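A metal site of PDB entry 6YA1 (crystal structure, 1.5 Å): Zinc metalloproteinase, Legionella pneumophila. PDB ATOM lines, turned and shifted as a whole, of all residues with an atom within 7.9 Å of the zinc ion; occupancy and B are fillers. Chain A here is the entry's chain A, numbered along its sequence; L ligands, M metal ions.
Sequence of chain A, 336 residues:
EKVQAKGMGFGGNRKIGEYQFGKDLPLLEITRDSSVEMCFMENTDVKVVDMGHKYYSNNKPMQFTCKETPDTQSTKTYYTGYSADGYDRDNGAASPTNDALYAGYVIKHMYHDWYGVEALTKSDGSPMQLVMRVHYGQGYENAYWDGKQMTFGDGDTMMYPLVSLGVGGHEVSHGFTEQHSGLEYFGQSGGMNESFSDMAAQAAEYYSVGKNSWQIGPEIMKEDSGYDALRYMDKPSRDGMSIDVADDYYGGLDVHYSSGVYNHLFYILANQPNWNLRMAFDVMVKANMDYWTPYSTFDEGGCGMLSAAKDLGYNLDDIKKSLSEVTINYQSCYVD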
ATOM      1  N   ASN A 142     -36.802  -1.780  -2.687  1.00  0.00           N
ATOM      2  CA  ASN A 142     -35.812  -1.150  -3.545  1.00  0.00           C
ATOM      3  C   ASN A 142     -34.608  -0.736  -2.694  1.00  0.00           C
ATOM      4  O   ASN A 142     -34.662  -0.733  -1.452  1.00  0.00           O
ATOM      5  CB  ASN A 142     -36.409   0.108  -4.209  1.00  0.00           C
ATOM      6  CG  ASN A 142     -35.548   0.669  -5.315  1.00  0.00           C
ATOM      7  OD1 ASN A 142     -34.995  -0.074  -6.123  1.00  0.00           O
ATOM      8  ND2 ASN A 142     -35.452   2.006  -5.374  1.00  0.00           N
ATOM      9  N   ALA A 143     -33.538  -0.376  -3.380  1.00  0.00           N
ATOM     10  CA  ALA A 143     -32.339   0.197  -2.792  1.00  0.00           C
ATOM     11  C   ALA A 143     -31.774   1.154  -3.830  1.00  0.00           C
ATOM     12  O   ALA A 143     -31.953   0.925  -5.030  1.00  0.00           O
ATOM     13  CB  ALA A 143     -31.316  -0.891  -2.492  1.00  0.00           C
ATOM     14  N   TYR A 144     -31.084   2.202  -3.402  1.00  0.00           N
ATOM     15  CA  TYR A 144     -30.561   3.144  -4.393  1.00  0.00           C
ATOM     16  C   TYR A 144     -29.414   3.971  -3.853  1.00  0.00           C
ATOM     17  O   TYR A 144     -29.205   4.099  -2.636  1.00  0.00           O
ATOM     18  CB  TYR A 144     -31.685   4.055  -4.917  1.00  0.00           C
ATOM     19  CG  TYR A 144     -32.256   4.997  -3.888  1.00  0.00           C
ATOM     20  CD1 TYR A 144     -33.265   4.589  -3.024  1.00  0.00           C
ATOM     21  CD2 TYR A 144     -31.855   6.309  -3.814  1.00  0.00           C
ATOM     22  CE1 TYR A 144     -33.838   5.459  -2.084  1.00  0.00           C
ATOM     23  CE2 TYR A 144     -32.417   7.198  -2.863  1.00  0.00           C
ATOM     24  CZ  TYR A 144     -33.387   6.740  -2.014  1.00  0.00           C
ATOM     25  OH  TYR A 144     -33.976   7.555  -1.065  1.00  0.00           O
ATOM     26  N   TRP A 145     -28.675   4.561  -4.806  1.00  0.00           N
ATOM     27  CA  TRP A 145     -27.645   5.568  -4.578  1.00  0.00           C
ATOM     28  C   TRP A 145     -28.199   6.933  -4.963  1.00  0.00           C
ATOM     29  O   TRP A 145     -28.861   7.072  -5.988  1.00  0.00           O
ATOM     30  CB  TRP A 145     -26.435   5.223  -5.463  1.00  0.00           C
ATOM     31  CG  TRP A 145     -25.441   6.335  -5.674  1.00  0.00           C
ATOM     32  CD1 TRP A 145     -25.341   7.118  -6.793  1.00  0.00           C
ATOM     33  CD2 TRP A 145     -24.408   6.773  -4.775  1.00  0.00           C
ATOM     34  NE1 TRP A 145     -24.308   8.018  -6.646  1.00  0.00           N
ATOM     35  CE2 TRP A 145     -23.718   7.828  -5.417  1.00  0.00           C
ATOM     36  CE3 TRP A 145     -23.974   6.369  -3.510  1.00  0.00           C
ATOM     37  CZ2 TRP A 145     -22.635   8.488  -4.829  1.00  0.00           C
ATOM     38  CZ3 TRP A 145     -22.900   7.049  -2.917  1.00  0.00           C
ATOM     39  CH2 TRP A 145     -22.249   8.093  -3.588  1.00  0.00           C
ATOM     40  N   VAL A 167     -26.121  -6.599  -2.993  1.00  0.00           N
ATOM     41  CA  VAL A 167     -26.878  -5.353  -3.128  1.00  0.00           C
ATOM     42  C   VAL A 167     -26.068  -4.181  -2.600  1.00  0.00           C
ATOM     43  O   VAL A 167     -26.063  -3.102  -3.192  1.00  0.00           O
ATOM     44  CB  VAL A 167     -28.254  -5.442  -2.467  1.00  0.00           C
ATOM     45  CG1 VAL A 167     -28.989  -4.116  -2.576  1.00  0.00           C
ATOM     46  CG2 VAL A 167     -29.112  -6.537  -3.098  1.00  0.00           C
ATOM     47  N   HIS A 170     -23.535  -3.356  -5.214  1.00  0.00           N
ATOM     48  CA  HIS A 170     -24.159  -2.701  -6.357  1.00  0.00           C
ATOM     49  C   HIS A 170     -24.364  -1.218  -6.071  1.00  0.00           C
ATOM     50  O   HIS A 170     -23.995  -0.356  -6.877  1.00  0.00           O
ATOM     51  CB  HIS A 170     -25.479  -3.434  -6.633  1.00  0.00           C
ATOM     52  CG  HIS A 170     -26.279  -2.852  -7.736  1.00  0.00           C
ATOM     53  ND1 HIS A 170     -26.445  -3.480  -8.950  1.00  0.00           N
ATOM     54  CD2 HIS A 170     -26.947  -1.676  -7.825  1.00  0.00           C
ATOM     55  CE1 HIS A 170     -27.180  -2.733  -9.741  1.00  0.00           C
ATOM     56  NE2 HIS A 170     -27.508  -1.646  -9.062  1.00  0.00           N
ATOM     57  N   GLU A 171     -24.931  -0.904  -4.901  1.00  0.00           N
ATOM     58  CA  GLU A 171     -25.273   0.487  -4.601  1.00  0.00           C
ATOM     59  C   GLU A 171     -24.027   1.345  -4.379  1.00  0.00           C
ATOM     60  O   GLU A 171     -23.949   2.484  -4.886  1.00  0.00           O
ATOM     61  CB  GLU A 171     -26.220   0.573  -3.432  1.00  0.00           C
ATOM     62  CG  GLU A 171     -27.571  -0.105  -3.619  1.00  0.00           C
ATOM     63  CD  GLU A 171     -28.327   0.357  -4.854  1.00  0.00           C
ATOM     64  OE1 GLU A 171     -28.035   1.448  -5.389  1.00  0.00           O
ATOM     65  OE2 GLU A 171     -29.214  -0.400  -5.323  1.00  0.00           O
ATOM     66  N   SER A 173     -21.230   0.901  -5.652  1.00  0.00           N
ATOM     67  CA  SER A 173     -20.546   1.020  -6.929  1.00  0.00           C
ATOM     68  C   SER A 173     -21.189   2.024  -7.876  1.00  0.00           C
ATOM     69  O   SER A 173     -20.519   2.503  -8.796  1.00  0.00           O
ATOM     70  CB  SER A 173     -20.371  -0.373  -7.555  1.00  0.00           C
ATOM     71  OG  SER A 173     -19.486  -1.162  -6.759  1.00  0.00           O
ATOM     72  N   HIS A 174     -22.463   2.352  -7.691  1.00  0.00           N
ATOM     73  CA  HIS A 174     -23.029   3.507  -8.372  1.00  0.00           C
ATOM     74  C   HIS A 174     -22.287   4.763  -7.994  1.00  0.00           C
ATOM     75  O   HIS A 174     -22.032   5.629  -8.854  1.00  0.00           O
ATOM     76  CB  HIS A 174     -24.488   3.615  -7.988  1.00  0.00           C
ATOM     77  CG  HIS A 174     -25.394   2.797  -8.819  1.00  0.00           C
ATOM     78  ND1 HIS A 174     -25.283   2.720 -10.195  1.00  0.00           N
ATOM     79  CD2 HIS A 174     -26.454   2.040  -8.471  1.00  0.00           C
ATOM     80  CE1 HIS A 174     -26.258   1.962 -10.667  1.00  0.00           C
ATOM     81  NE2 HIS A 174     -26.956   1.526  -9.640  1.00  0.00           N
ATOM     82  N   TYR A 185     -27.020   7.983 -16.176  1.00  0.00           N
ATOM     83  CA  TYR A 185     -27.946   6.919 -15.799  1.00  0.00           C
ATOM     84  C   TYR A 185     -29.158   6.784 -16.734  1.00  0.00           C
ATOM     85  O   TYR A 185     -30.293   6.614 -16.278  1.00  0.00           O
ATOM     86  CB  TYR A 185     -28.367   7.082 -14.335  1.00  0.00           C
ATOM     87  CG  TYR A 185     -28.881   5.818 -13.656  1.00  0.00           C
ATOM     88  CD1 TYR A 185     -28.112   4.658 -13.606  1.00  0.00           C
ATOM     89  CD2 TYR A 185     -30.140   5.769 -13.081  1.00  0.00           C
ATOM     90  CE1 TYR A 185     -28.587   3.504 -12.990  1.00  0.00           C
ATOM     91  CE2 TYR A 185     -30.608   4.637 -12.483  1.00  0.00           C
ATOM     92  CZ  TYR A 185     -29.830   3.508 -12.441  1.00  0.00           C
ATOM     93  OH  TYR A 185     -30.350   2.400 -11.834  1.00  0.00           O
ATOM     94  N   GLY A 190     -26.328   4.263 -19.254  1.00  0.00           N
ATOM     95  CA  GLY A 190     -27.027   3.842 -18.061  1.00  0.00           C
ATOM     96  C   GLY A 190     -27.106   2.339 -17.923  1.00  0.00           C
ATOM     97  O   GLY A 190     -27.084   1.815 -16.797  1.00  0.00           O
ATOM     98  N   ASN A 193     -23.789   1.535 -16.601  1.00  0.00           N
ATOM     99  CA  ASN A 193     -23.705   1.898 -15.190  1.00  0.00           C
ATOM    100  C   ASN A 193     -24.315   0.810 -14.331  1.00  0.00           C
ATOM    101  O   ASN A 193     -23.682   0.292 -13.408  1.00  0.00           O
ATOM    102  CB  ASN A 193     -24.425   3.227 -15.045  1.00  0.00           C
ATOM    103  CG  ASN A 193     -24.327   3.819 -13.656  1.00  0.00           C
ATOM    104  OD1 ASN A 193     -24.411   3.106 -12.673  1.00  0.00           O
ATOM    105  ND2 ASN A 193     -24.158   5.146 -13.570  1.00  0.00           N
ATOM    106  N   GLU A 194     -25.551   0.425 -14.652  1.00  0.00           N
ATOM    107  CA  GLU A 194     -26.185  -0.718 -14.016  1.00  0.00           C
ATOM    108  C   GLU A 194     -25.303  -1.957 -14.053  1.00  0.00           C
ATOM    109  O   GLU A 194     -25.098  -2.630 -13.027  1.00  0.00           O
ATOM    110  CB  GLU A 194     -27.541  -1.001 -14.698  1.00  0.00           C
ATOM    111  CG  GLU A 194     -28.714  -0.286 -14.044  1.00  0.00           C
ATOM    112  CD  GLU A 194     -28.777  -0.599 -12.544  1.00  0.00           C
ATOM    113  OE1 GLU A 194     -28.549   0.336 -11.760  1.00  0.00           O
ATOM    114  OE2 GLU A 194     -28.954  -1.793 -12.175  1.00  0.00           O
ATOM    115  N   SER A 195     -24.735  -2.271 -15.224  1.00  0.00           N
ATOM    116  CA  SER A 195     -23.952  -3.501 -15.321  1.00  0.00           C
ATOM    117  C   SER A 195     -22.727  -3.431 -14.429  1.00  0.00           C
ATOM    118  O   SER A 195     -22.357  -4.427 -13.805  1.00  0.00           O
ATOM    119  CB  SER A 195     -23.478  -3.758 -16.750  1.00  0.00           C
ATOM    120  OG  SER A 195     -24.547  -3.907 -17.665  1.00  0.00           O
ATOM    121  N   SER A 197     -22.331  -2.010 -11.706  1.00  0.00           N
ATOM    122  CA  SER A 197     -22.745  -2.281 -10.336  1.00  0.00           C
ATOM    123  C   SER A 197     -23.076  -3.758 -10.129  1.00  0.00           C
ATOM    124  O   SER A 197     -22.835  -4.294  -9.033  1.00  0.00           O
ATOM    125  CB  SER A 197     -23.915  -1.374  -9.935  1.00  0.00           C
ATOM    126  OG  SER A 197     -23.468  -0.050  -9.600  1.00  0.00           O
ATOM    127  N   ASP A 198     -23.657  -4.429 -11.129  1.00  0.00           N
ATOM    128  CA  ASP A 198     -23.898  -5.859 -11.009  1.00  0.00           C
ATOM    129  C   ASP A 198     -22.583  -6.648 -11.015  1.00  0.00           C
ATOM    130  O   ASP A 198     -22.460  -7.653 -10.314  1.00  0.00           O
ATOM    131  CB  ASP A 198     -24.816  -6.330 -12.118  1.00  0.00           C
ATOM    132  CG  ASP A 198     -26.273  -5.895 -11.918  1.00  0.00           C
ATOM    133  OD1 ASP A 198     -26.671  -5.503 -10.783  1.00  0.00           O
ATOM    134  OD2 ASP A 198     -27.042  -6.001 -12.910  1.00  0.00           O
ATOM    135  N   ARG A 231     -31.865 -10.795 -11.474  1.00  0.00           N
ATOM    136  CA  ARG A 231     -31.243 -10.906 -12.781  1.00  0.00           C
ATOM    137  C   ARG A 231     -30.272 -12.064 -12.832  1.00  0.00           C
ATOM    138  O   ARG A 231     -29.723 -12.503 -11.811  1.00  0.00           O
ATOM    139  CB  ARG A 231     -30.445  -9.639 -13.136  1.00  0.00           C
ATOM    140  CG  ARG A 231     -31.280  -8.448 -13.368  1.00  0.00           C
ATOM    141  CD  ARG A 231     -30.385  -7.246 -13.620  1.00  0.00           C
ATOM    142  NE  ARG A 231     -29.735  -6.600 -12.479  1.00  0.00           N
ATOM    143  CZ  ARG A 231     -30.346  -5.795 -11.617  1.00  0.00           C
ATOM    144  NH1 ARG A 231     -31.653  -5.595 -11.732  1.00  0.00           N
ATOM    145  NH2 ARG A 231     -29.650  -5.213 -10.650  1.00  0.00           N
ATOM    146  N   VAL A 255     -32.835   0.733 -17.936  1.00  0.00           N
ATOM    147  CA  VAL A 255     -31.443   0.441 -17.641  1.00  0.00           C
ATOM    148  C   VAL A 255     -31.297  -0.901 -16.940  1.00  0.00           C
ATOM    149  O   VAL A 255     -30.235  -1.525 -16.999  1.00  0.00           O
ATOM    150  CB  VAL A 255     -30.774   1.563 -16.818  1.00  0.00           C
ATOM    151  CG1 VAL A 255     -30.685   2.895 -17.606  1.00  0.00           C
ATOM    152  CG2 VAL A 255     -31.480   1.772 -15.454  1.00  0.00           C
ATOM    153  N   HIS A 256     -32.351  -1.359 -16.237  1.00  0.00           N
ATOM    154  CA  HIS A 256     -32.276  -2.639 -15.535  1.00  0.00           C
ATOM    155  C   HIS A 256     -32.443  -3.822 -16.473  1.00  0.00           C
ATOM    156  O   HIS A 256     -32.276  -4.961 -16.037  1.00  0.00           O
ATOM    157  CB  HIS A 256     -33.306  -2.754 -14.432  1.00  0.00           C
ATOM    158  CG  HIS A 256     -33.035  -1.860 -13.276  1.00  0.00           C
ATOM    159  ND1 HIS A 256     -33.895  -0.847 -12.921  1.00  0.00           N
ATOM    160  CD2 HIS A 256     -31.993  -1.787 -12.416  1.00  0.00           C
ATOM    161  CE1 HIS A 256     -33.410  -0.198 -11.886  1.00  0.00           C
ATOM    162  NE2 HIS A 256     -32.249  -0.739 -11.560  1.00  0.00           N
HETATM  163  C1  LIG L   1     -30.602   0.383  -8.539  1.00  0.00           C
HETATM  164  O1  LIG L   1     -29.787   0.621  -7.611  1.00  0.00           O
HETATM  165  O2  LIG L   1     -30.399  -0.023  -9.683  1.00  0.00           O
HETATM  166  C2  LIG L   1     -32.036   0.645  -8.267  1.00  0.00           C
HETATM  167 ZN    ZN M   1     -28.471   0.024  -9.829  1.00  0.00          ZN
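ND1 of His 174 sits at hydrogen-bond distance from OD1 of Asn 193 (2.7 Å).
O of His 170 is in hydrogen-bond range of OG of Ser 197, 2.8 Å away.
A ring nitrogen (ND1) of His 170 lies within hydrogen-bond range of the side-chain carboxylate of Asp 198, at 2.7 Å.
The guanidinium group of Arg 231 lies within salt-bridge range of the side-chain carboxylate of Glu 194 (3.8 Å).
The backbone NH (N) of His 174 sits at hydrogen-bond distance from the side-chain hydroxyl (OG) of Ser 197.
The side-chain carboxylate (OE1) of Glu 194 lies close to the side-chain hydroxyl (OH) of Tyr 185, at 2.7 Å.
Tyr 185 touches the zinc ion (OH to ZN, 3.6 Å).
Within 4 Å of the zinc ion: His 170, His 174, Tyr 185 and Glu 194.
The nearest printed residue that does not touch the zinc ion is His 256 (4.2 Å).
The zinc ion is bound by O2 of the ligand, OE1 of Glu 194, NE2 of His 170 and NE2 of His 174.
The zinc ion has four donor atoms within binding distance.
Slightly farther from the zinc ion lies an oxygen (O1) of the ligand (2.6 Å).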
